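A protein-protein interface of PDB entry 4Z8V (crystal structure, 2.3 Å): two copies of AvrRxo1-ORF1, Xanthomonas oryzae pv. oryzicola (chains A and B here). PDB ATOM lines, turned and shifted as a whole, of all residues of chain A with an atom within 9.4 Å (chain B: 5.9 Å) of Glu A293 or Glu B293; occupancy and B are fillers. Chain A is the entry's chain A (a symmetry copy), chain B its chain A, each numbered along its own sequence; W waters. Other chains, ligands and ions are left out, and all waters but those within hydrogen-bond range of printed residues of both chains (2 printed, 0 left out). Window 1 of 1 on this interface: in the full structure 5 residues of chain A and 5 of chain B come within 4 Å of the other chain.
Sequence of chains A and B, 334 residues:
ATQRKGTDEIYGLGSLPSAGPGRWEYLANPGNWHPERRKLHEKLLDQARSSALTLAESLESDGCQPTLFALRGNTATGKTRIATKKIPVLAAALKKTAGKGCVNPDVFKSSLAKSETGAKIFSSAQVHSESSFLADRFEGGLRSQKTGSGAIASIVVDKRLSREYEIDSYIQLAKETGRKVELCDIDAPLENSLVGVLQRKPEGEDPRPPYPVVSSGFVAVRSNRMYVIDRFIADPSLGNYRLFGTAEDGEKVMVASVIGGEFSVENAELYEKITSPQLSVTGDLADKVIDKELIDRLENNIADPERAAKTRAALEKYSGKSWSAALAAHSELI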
ATOM      1  N   GLU A 191     -27.968  -3.491   2.943  1.00  0.00           N
ATOM      2  CA  GLU A 191     -27.367  -2.961   1.718  1.00  0.00           C
ATOM      3  C   GLU A 191     -27.699  -3.807   0.499  1.00  0.00           C
ATOM      4  O   GLU A 191     -27.833  -3.275  -0.607  1.00  0.00           O
ATOM      5  CB  GLU A 191     -25.846  -2.809   1.854  1.00  0.00           C
ATOM      6  CG  GLU A 191     -25.418  -1.515   2.511  1.00  0.00           C
ATOM      7  CD  GLU A 191     -23.970  -1.135   2.207  1.00  0.00           C
ATOM      8  OE1 GLU A 191     -23.093  -2.042   2.185  1.00  0.00           O
ATOM      9  OE2 GLU A 191     -23.723   0.078   1.988  1.00  0.00           O
ATOM     10  N   LYS A 288     -25.022   7.504   3.795  1.00  0.00           N
ATOM     11  CA  LYS A 288     -23.808   6.978   3.180  1.00  0.00           C
ATOM     12  C   LYS A 288     -23.857   7.244   1.669  1.00  0.00           C
ATOM     13  O   LYS A 288     -24.896   7.021   1.022  1.00  0.00           O
ATOM     14  CB  LYS A 288     -23.663   5.487   3.504  1.00  0.00           C
ATOM     15  CG  LYS A 288     -22.582   4.751   2.740  1.00  0.00           C
ATOM     16  CD  LYS A 288     -21.189   5.325   2.985  1.00  0.00           C
ATOM     17  CE  LYS A 288     -20.167   4.594   2.115  1.00  0.00           C
ATOM     18  NZ  LYS A 288     -18.918   5.389   1.887  1.00  0.00           N
ATOM     19  N   VAL A 289     -22.764   7.788   1.125  1.00  0.00           N
ATOM     20  CA  VAL A 289     -22.739   8.203  -0.282  1.00  0.00           C
ATOM     21  C   VAL A 289     -22.286   7.051  -1.174  1.00  0.00           C
ATOM     22  O   VAL A 289     -21.335   6.351  -0.853  1.00  0.00           O
ATOM     23  CB  VAL A 289     -21.851   9.465  -0.506  1.00  0.00           C
ATOM     24  CG1 VAL A 289     -21.674   9.740  -1.991  1.00  0.00           C
ATOM     25  CG2 VAL A 289     -22.461  10.703   0.187  1.00  0.00           C
ATOM     26  N   ILE A 290     -23.006   6.838  -2.272  1.00  0.00           N
ATOM     27  CA  ILE A 290     -22.614   5.859  -3.275  1.00  0.00           C
ATOM     28  C   ILE A 290     -21.438   6.426  -4.072  1.00  0.00           C
ATOM     29  O   ILE A 290     -21.606   7.325  -4.909  1.00  0.00           O
ATOM     30  CB  ILE A 290     -23.779   5.539  -4.232  1.00  0.00           C
ATOM     31  CG1 ILE A 290     -24.940   4.884  -3.474  1.00  0.00           C
ATOM     32  CG2 ILE A 290     -23.315   4.630  -5.368  1.00  0.00           C
ATOM     33  CD1 ILE A 290     -26.269   4.824  -4.268  1.00  0.00           C
ATOM     34  N   ASP A 291     -20.240   5.932  -3.786  1.00  0.00           N
ATOM     35  CA  ASP A 291     -19.069   6.352  -4.540  1.00  0.00           C
ATOM     36  C   ASP A 291     -18.359   5.129  -5.110  1.00  0.00           C
ATOM     37  O   ASP A 291     -18.851   4.003  -4.971  1.00  0.00           O
ATOM     38  CB  ASP A 291     -18.130   7.215  -3.687  1.00  0.00           C
ATOM     39  CG  ASP A 291     -17.757   6.557  -2.378  1.00  0.00           C
ATOM     40  OD1 ASP A 291     -18.042   5.352  -2.204  1.00  0.00           O
ATOM     41  OD2 ASP A 291     -17.156   7.240  -1.515  1.00  0.00           O
ATOM     42  N   LYS A 292     -17.211   5.351  -5.745  1.00  0.00           N
ATOM     43  CA  LYS A 292     -16.503   4.284  -6.432  1.00  0.00           C
ATOM     44  C   LYS A 292     -16.152   3.170  -5.449  1.00  0.00           C
ATOM     45  O   LYS A 292     -16.286   1.975  -5.750  1.00  0.00           O
ATOM     46  CB  LYS A 292     -15.242   4.830  -7.101  1.00  0.00           C
ATOM     47  CG  LYS A 292     -14.497   3.820  -7.970  1.00  0.00           C
ATOM     48  CD  LYS A 292     -13.244   4.449  -8.565  1.00  0.00           C
ATOM     49  CE  LYS A 292     -12.447   3.453  -9.404  1.00  0.00           C
ATOM     50  NZ  LYS A 292     -11.660   2.501  -8.577  1.00  0.00           N
ATOM     51  N   GLU A 293     -15.727   3.572  -4.262  1.00  0.00           N
ATOM     52  CA  GLU A 293     -15.353   2.610  -3.246  1.00  0.00           C
ATOM     53  C   GLU A 293     -16.527   1.707  -2.839  1.00  0.00           C
ATOM     54  O   GLU A 293     -16.384   0.485  -2.846  1.00  0.00           O
ATOM     55  CB  GLU A 293     -14.722   3.311  -2.031  1.00  0.00           C
ATOM     56  CG  GLU A 293     -14.485   2.387  -0.836  1.00  0.00           C
ATOM     57  CD  GLU A 293     -14.014   0.992  -1.241  1.00  0.00           C
ATOM     58  OE1 GLU A 293     -14.577   0.005  -0.710  1.00  0.00           O
ATOM     59  OE2 GLU A 293     -13.106   0.876  -2.102  1.00  0.00           O
ATOM     60  N   LEU A 294     -17.673   2.294  -2.496  1.00  0.00           N
ATOM     61  CA  LEU A 294     -18.853   1.489  -2.168  1.00  0.00           C
ATOM     62  C   LEU A 294     -19.152   0.504  -3.302  1.00  0.00           C
ATOM     63  O   LEU A 294     -19.325  -0.695  -3.066  1.00  0.00           O
ATOM     64  CB  LEU A 294     -20.070   2.376  -1.865  1.00  0.00           C
ATOM     65  CG  LEU A 294     -21.394   1.689  -1.490  1.00  0.00           C
ATOM     66  CD1 LEU A 294     -22.153   2.486  -0.442  1.00  0.00           C
ATOM     67  CD2 LEU A 294     -22.289   1.526  -2.691  1.00  0.00           C
ATOM     68  N   ILE A 295     -19.171   1.007  -4.535  1.00  0.00           N
ATOM     69  CA  ILE A 295     -19.470   0.163  -5.689  1.00  0.00           C
ATOM     70  C   ILE A 295     -18.466  -0.971  -5.831  1.00  0.00           C
ATOM     71  O   ILE A 295     -18.865  -2.118  -6.012  1.00  0.00           O
ATOM     72  CB  ILE A 295     -19.516   0.955  -7.004  1.00  0.00           C
ATOM     73  CG1 ILE A 295     -20.583   2.042  -6.945  1.00  0.00           C
ATOM     74  CG2 ILE A 295     -19.807   0.027  -8.157  1.00  0.00           C
ATOM     75  CD1 ILE A 295     -20.670   2.881  -8.200  1.00  0.00           C
ATOM     76  N   ASP A 296     -17.172  -0.652  -5.743  1.00  0.00           N
ATOM     77  CA  ASP A 296     -16.135  -1.679  -5.832  1.00  0.00           C
ATOM     78  C   ASP A 296     -16.263  -2.720  -4.721  1.00  0.00           C
ATOM     79  O   ASP A 296     -16.121  -3.915  -4.962  1.00  0.00           O
ATOM     80  CB  ASP A 296     -14.737  -1.060  -5.756  1.00  0.00           C
ATOM     81  CG  ASP A 296     -14.387  -0.227  -6.973  1.00  0.00           C
ATOM     82  OD1 ASP A 296     -15.114  -0.293  -7.993  1.00  0.00           O
ATOM     83  OD2 ASP A 296     -13.364   0.497  -6.899  1.00  0.00           O
ATOM     84  N   ARG A 297     -16.494  -2.251  -3.501  1.00  0.00           N
ATOM     85  CA  ARG A 297     -16.640  -3.130  -2.346  1.00  0.00           C
ATOM     86  C   ARG A 297     -17.767  -4.144  -2.574  1.00  0.00           C
ATOM     87  O   ARG A 297     -17.592  -5.337  -2.330  1.00  0.00           O
ATOM     88  CB  ARG A 297     -16.907  -2.302  -1.084  1.00  0.00           C
ATOM     89  CG  ARG A 297     -17.215  -3.123   0.154  1.00  0.00           C
ATOM     90  CD  ARG A 297     -17.195  -2.280   1.439  1.00  0.00           C
ATOM     91  NE  ARG A 297     -18.168  -1.180   1.481  1.00  0.00           N
ATOM     92  CZ  ARG A 297     -19.445  -1.302   1.862  1.00  0.00           C
ATOM     93  NH1 ARG A 297     -19.936  -2.488   2.201  1.00  0.00           N
ATOM     94  NH2 ARG A 297     -20.250  -0.239   1.896  1.00  0.00           N
ATOM     95  N   LEU A 298     -18.909  -3.672  -3.069  1.00  0.00           N
ATOM     96  CA  LEU A 298     -20.052  -4.547  -3.285  1.00  0.00           C
ATOM     97  C   LEU A 298     -19.772  -5.518  -4.426  1.00  0.00           C
ATOM     98  O   LEU A 298     -20.182  -6.690  -4.379  1.00  0.00           O
ATOM     99  CB  LEU A 298     -21.316  -3.726  -3.538  1.00  0.00           C
ATOM    100  CG  LEU A 298     -21.819  -2.966  -2.307  1.00  0.00           C
ATOM    101  CD1 LEU A 298     -22.977  -2.063  -2.657  1.00  0.00           C
ATOM    102  CD2 LEU A 298     -22.225  -3.925  -1.195  1.00  0.00           C
ATOM    103  N   GLU A 299     -19.047  -5.036  -5.433  1.00  0.00           N
ATOM    104  CA  GLU A 299     -18.632  -5.860  -6.570  1.00  0.00           C
ATOM    105  C   GLU A 299     -17.644  -6.959  -6.170  1.00  0.00           C
ATOM    106  O   GLU A 299     -17.669  -8.066  -6.720  1.00  0.00           O
ATOM    107  CB  GLU A 299     -18.004  -4.969  -7.644  1.00  0.00           C
ATOM    108  CG  GLU A 299     -19.007  -4.088  -8.359  1.00  0.00           C
ATOM    109  CD  GLU A 299     -19.882  -4.873  -9.304  1.00  0.00           C
ATOM    110  OE1 GLU A 299     -19.328  -5.469 -10.256  1.00  0.00           O
ATOM    111  OE2 GLU A 299     -21.119  -4.884  -9.103  1.00  0.00           O
ATOM    112  N   ASN A 300     -16.782  -6.642  -5.209  1.00  0.00           N
ATOM    113  CA  ASN A 300     -15.771  -7.575  -4.717  1.00  0.00           C
ATOM    114  C   ASN A 300     -16.342  -8.891  -4.169  1.00  0.00           C
ATOM    115  O   ASN A 300     -15.617  -9.891  -4.050  1.00  0.00           O
ATOM    116  CB  ASN A 300     -14.921  -6.886  -3.646  1.00  0.00           C
ATOM    117  CG  ASN A 300     -13.679  -7.675  -3.279  1.00  0.00           C
ATOM    118  OD1 ASN A 300     -13.540  -8.179  -2.151  1.00  0.00           O
ATOM    119  ND2 ASN A 300     -12.761  -7.784  -4.230  1.00  0.00           N
ATOM    120  N   ASN A 301     -17.629  -8.898  -3.826  1.00  0.00           N
ATOM    121  CA  ASN A 301     -18.254 -10.117  -3.327  1.00  0.00           C
ATOM    122  C   ASN A 301     -19.355 -10.616  -4.240  1.00  0.00           C
ATOM    123  O   ASN A 301     -20.236 -11.373  -3.804  1.00  0.00           O
ATOM    124  CB  ASN A 301     -18.791  -9.929  -1.909  1.00  0.00           C
ATOM    125  CG  ASN A 301     -17.691  -9.698  -0.893  1.00  0.00           C
ATOM    126  OD1 ASN A 301     -17.603  -8.623  -0.297  1.00  0.00           O
ATOM    127  ND2 ASN A 301     -16.852 -10.709  -0.681  1.00  0.00           N
ATOM    128  N   LEU A 315     -26.049   1.111  -9.463  1.00  0.00           N
ATOM    129  CA  LEU A 315     -25.313   2.020  -8.584  1.00  0.00           C
ATOM    130  C   LEU A 315     -24.676   3.222  -9.299  1.00  0.00           C
ATOM    131  O   LEU A 315     -24.653   4.332  -8.751  1.00  0.00           O
ATOM    132  CB  LEU A 315     -24.225   1.258  -7.814  1.00  0.00           C
ATOM    133  CG  LEU A 315     -24.688   0.170  -6.846  1.00  0.00           C
ATOM    134  CD1 LEU A 315     -23.505  -0.569  -6.231  1.00  0.00           C
ATOM    135  CD2 LEU A 315     -25.584   0.762  -5.755  1.00  0.00           C
ATOM    136  N   SER A 319     -24.388   7.383  -8.535  1.00  0.00           N
ATOM    137  CA  SER A 319     -23.100   7.745  -7.941  1.00  0.00           C
ATOM    138  C   SER A 319     -23.129   9.183  -7.391  1.00  0.00           C
ATOM    139  O   SER A 319     -23.787  10.070  -7.945  1.00  0.00           O
ATOM    140  CB  SER A 319     -21.961   7.566  -8.949  1.00  0.00           C
ATOM    141  OG  SER A 319     -22.306   8.146 -10.202  1.00  0.00           O
ATOM    142  N   GLY A 320     -22.468   9.396  -6.264  1.00  0.00           N
ATOM    143  CA  GLY A 320     -22.492  10.704  -5.632  1.00  0.00           C
ATOM    144  C   GLY A 320     -23.749  10.972  -4.824  1.00  0.00           C
ATOM    145  O   GLY A 320     -23.839  11.995  -4.146  1.00  0.00           O
ATOM    146  N   ASP B 291      -6.510  -7.793   0.161  1.00  0.00           N
ATOM    147  CA  ASP B 291      -6.550  -7.716  -1.291  1.00  0.00           C
ATOM    148  C   ASP B 291      -6.745  -6.267  -1.724  1.00  0.00           C
ATOM    149  O   ASP B 291      -6.757  -5.363  -0.880  1.00  0.00           O
ATOM    150  CB  ASP B 291      -7.627  -8.639  -1.875  1.00  0.00           C
ATOM    151  CG  ASP B 291      -8.988  -8.415  -1.257  1.00  0.00           C
ATOM    152  OD1 ASP B 291      -9.165  -7.414  -0.530  1.00  0.00           O
ATOM    153  OD2 ASP B 291      -9.901  -9.237  -1.510  1.00  0.00           O
ATOM    154  N   LYS B 292      -6.900  -6.051  -3.028  1.00  0.00           N
ATOM    155  CA  LYS B 292      -6.975  -4.706  -3.573  1.00  0.00           C
ATOM    156  C   LYS B 292      -8.149  -3.954  -2.952  1.00  0.00           C
ATOM    157  O   LYS B 292      -8.044  -2.773  -2.593  1.00  0.00           O
ATOM    158  CB  LYS B 292      -7.113  -4.759  -5.095  1.00  0.00           C
ATOM    159  CG  LYS B 292      -7.059  -3.397  -5.783  1.00  0.00           C
ATOM    160  CD  LYS B 292      -7.236  -3.553  -7.288  1.00  0.00           C
ATOM    161  CE  LYS B 292      -7.233  -2.206  -8.007  1.00  0.00           C
ATOM    162  NZ  LYS B 292      -8.519  -1.473  -7.862  1.00  0.00           N
ATOM    163  N   GLU B 293      -9.260  -4.658  -2.801  1.00  0.00           N
ATOM    164  CA  GLU B 293     -10.447  -4.053  -2.232  1.00  0.00           C
ATOM    165  C   GLU B 293     -10.219  -3.566  -0.793  1.00  0.00           C
ATOM    166  O   GLU B 293     -10.514  -2.411  -0.489  1.00  0.00           O
ATOM    167  CB  GLU B 293     -11.650  -5.006  -2.331  1.00  0.00           C
ATOM    168  CG  GLU B 293     -12.888  -4.522  -1.575  1.00  0.00           C
ATOM    169  CD  GLU B 293     -13.099  -3.013  -1.675  1.00  0.00           C
ATOM    170  OE1 GLU B 293     -13.350  -2.384  -0.619  1.00  0.00           O
ATOM    171  OE2 GLU B 293     -12.993  -2.451  -2.794  1.00  0.00           O
ATOM    172  N   LEU B 294      -9.696  -4.428   0.079  1.00  0.00           N
ATOM    173  CA  LEU B 294      -9.387  -4.005   1.448  1.00  0.00           C
ATOM    174  C   LEU B 294      -8.495  -2.760   1.427  1.00  0.00           C
ATOM    175  O   LEU B 294      -8.787  -1.765   2.097  1.00  0.00           O
ATOM    176  CB  LEU B 294      -8.737  -5.142   2.252  1.00  0.00           C
ATOM    177  CG  LEU B 294      -8.357  -4.870   3.717  1.00  0.00           C
ATOM    178  CD1 LEU B 294      -8.579  -6.098   4.583  1.00  0.00           C
ATOM    179  CD2 LEU B 294      -6.911  -4.464   3.844  1.00  0.00           C
ATOM    180  N   ILE B 295      -7.433  -2.804   0.625  1.00  0.00           N
ATOM    181  CA  ILE B 295      -6.501  -1.682   0.546  1.00  0.00           C
ATOM    182  C   ILE B 295      -7.192  -0.410   0.077  1.00  0.00           C
ATOM    183  O   ILE B 295      -7.014   0.640   0.687  1.00  0.00           O
ATOM    184  CB  ILE B 295      -5.308  -1.969  -0.377  1.00  0.00           C
ATOM    185  CG1 ILE B 295      -4.523  -3.180   0.113  1.00  0.00           C
ATOM    186  CG2 ILE B 295      -4.396  -0.768  -0.434  1.00  0.00           C
ATOM    187  CD1 ILE B 295      -3.343  -3.539  -0.762  1.00  0.00           C
ATOM    188  N   ASP B 296      -7.981  -0.506  -0.997  1.00  0.00           N
ATOM    189  CA  ASP B 296      -8.714   0.654  -1.501  1.00  0.00           C
ATOM    190  C   ASP B 296      -9.688   1.210  -0.464  1.00  0.00           C
ATOM    191  O   ASP B 296      -9.795   2.420  -0.290  1.00  0.00           O
ATOM    192  CB  ASP B 296      -9.503   0.303  -2.764  1.00  0.00           C
ATOM    193  CG  ASP B 296      -8.616   0.014  -3.959  1.00  0.00           C
ATOM    194  OD1 ASP B 296      -7.395   0.296  -3.901  1.00  0.00           O
ATOM    195  OD2 ASP B 296      -9.160  -0.500  -4.967  1.00  0.00           O
ATOM    196  N   ARG B 297     -10.419   0.318   0.193  1.00  0.00           N
ATOM    197  CA  ARG B 297     -11.388   0.707   1.213  1.00  0.00           C
ATOM    198  C   ARG B 297     -10.712   1.523   2.322  1.00  0.00           C
ATOM    199  O   ARG B 297     -11.218   2.570   2.722  1.00  0.00           O
ATOM    200  CB  ARG B 297     -12.067  -0.537   1.796  1.00  0.00           C
ATOM    201  CG  ARG B 297     -12.993  -0.259   2.965  1.00  0.00           C
ATOM    202  CD  ARG B 297     -13.860  -1.474   3.331  1.00  0.00           C
ATOM    203  NE  ARG B 297     -13.116  -2.675   3.735  1.00  0.00           N
ATOM    204  CZ  ARG B 297     -12.669  -2.918   4.973  1.00  0.00           C
ATOM    205  NH1 ARG B 297     -12.848  -2.026   5.940  1.00  0.00           N
ATOM    206  NH2 ARG B 297     -12.026  -4.051   5.254  1.00  0.00           N
ATOM    207  N   LEU B 298      -9.558   1.056   2.793  1.00  0.00           N
ATOM    208  CA  LEU B 298      -8.858   1.737   3.872  1.00  0.00           C
ATOM    209  C   LEU B 298      -8.306   3.073   3.391  1.00  0.00           C
ATOM    210  O   LEU B 298      -8.303   4.066   4.137  1.00  0.00           O
ATOM    211  CB  LEU B 298      -7.758   0.843   4.445  1.00  0.00           C
ATOM    212  CG  LEU B 298      -8.284  -0.369   5.220  1.00  0.00           C
ATOM    213  CD1 LEU B 298      -7.157  -1.286   5.631  1.00  0.00           C
ATOM    214  CD2 LEU B 298      -9.077   0.063   6.447  1.00  0.00           C
ATOM    215  N   ASN B 300      -9.686   4.905   1.033  1.00  0.00           N
ATOM    216  CA  ASN B 300     -10.841   5.774   0.821  1.00  0.00           C
ATOM    217  C   ASN B 300     -11.157   6.701   2.005  1.00  0.00           C
ATOM    218  O   ASN B 300     -11.861   7.710   1.844  1.00  0.00           O
ATOM    219  CB  ASN B 300     -12.065   4.921   0.481  1.00  0.00           C
ATOM    220  CG  ASN B 300     -13.235   5.742  -0.027  1.00  0.00           C
ATOM    221  OD1 ASN B 300     -14.288   5.845   0.627  1.00  0.00           O
ATOM    222  ND2 ASN B 300     -13.062   6.331  -1.202  1.00  0.00           N
HETATM  223  O   HOH W   1      -9.892  -7.288  -4.550  1.00  0.00           O
HETATM  224  O   HOH W   2     -14.446   6.487  -3.779  1.00  0.00           O
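Asn B300 touches Asp A291.
Asp B296 touches Glu A293 (CB to OE2, 3.7 Å).
Glu A293 touches Arg B297 (OE2 to N, 3.6 Å).
Glu A293 touches Asn B300.
CB of Asp A296 touches OE2 of Glu B293, at 3.7 Å.
Arg A297 touches Glu B293.
Arg A297 touches Arg B297.
Asn A300 touches Asp B291.
Asn A300 touches Glu B293 (CG to CB, 3.5 Å).
Printed residues of chain B within 4 Å of Glu A293: Glu B293, Asp B296, Arg B297 and Asn B300.
Glu B293 touches just these residues of chain A: Glu A293 (2.7 Å), Asp A296 (3.7 Å), Arg A297 (3.6 Å) and Asn A300 (3.5 Å).
Printed residues of chain A within 4 Å of Asp B291: Asn A300.
Of the printed residues of chain A, Arg B297 touches Glu A293 (3.6 Å) and Arg A297 (3.9 Å).
Of the printed residues of chain A, Asn B300 touches Asp A291 and Glu A293.
Of the printed residues of chain A, Asp B296 touches Glu A293.
Of the printed residues of chain B, Asp A296 touches Glu B293.
Leu B294 touches none of the printed residues of chain A.
The nearest printed residue of chain B that does not touch Glu A293 is Leu B298 (6.0 Å).
The nearest printed residue of chain A that does not touch Asn B300 is Lys A288 (4.8 Å).
The side-chain carboxylate (OE1) of Glu A293 sits close to the side-chain carboxylate (OE1) of Glu B293, 2.7 Å away.
Glu A293 touches Asp B296, and with the chains exchanged Asp A296 touches Glu B293.
Glu A293 touches Arg B297, and with the chains exchanged Arg A297 touches Glu B293.
Glu A293 touches Asn B300, and with the chains exchanged Asn A300 touches Glu B293.
Arg B297 touches its own counterpart, Arg A297.
Positions printed for both chains: 291, 292, 293, 294, 295, 296, 297, 298 and 300.
The backbone NH (N) of Leu B294 is in hydrogen-bond range of the side-chain carboxylate (OD1) of Asp B291.
The side-chain carboxylate (OD2) of Asp B296 is in salt-bridge range of the side-chain amino group (NZ) of Lys B292.
The guanidinium group of Arg A297 lies within salt-bridge range of the side-chain carboxylate of Glu A191.
The side-chain carboxylate (OD1) of Asp A291 lies within hydrogen-bond range of the backbone NH (N) of Leu A294, 3.1 Å away.
The side-chain amino group (NZ) of Lys A292 lies within salt-bridge range of the side-chain carboxylate (OD2) of Asp A296 (3.1 Å).
Of the 9 printed residues of chain B, 5 touch a printed residue of chain A.
Along chain B the printed residues that touch a printed residue of chain A span positions 291 to 300.
Among the printed residues, no Asp or Glu carboxylate lies within 4 Å of a Lys or Arg side-chain nitrogen of the other chain.
Water W1 lies within hydrogen-bond range of the side-chain amide nitrogen (ND2) of Asn A300 (2.9 Å) and the backbone NH (N) of Glu B293 (3.2 Å).
Water W2 lies within hydrogen-bond range of the side-chain amide nitrogen of Asn B300 (2.9 Å) and the backbone NH of Glu A293 (3.2 Å).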
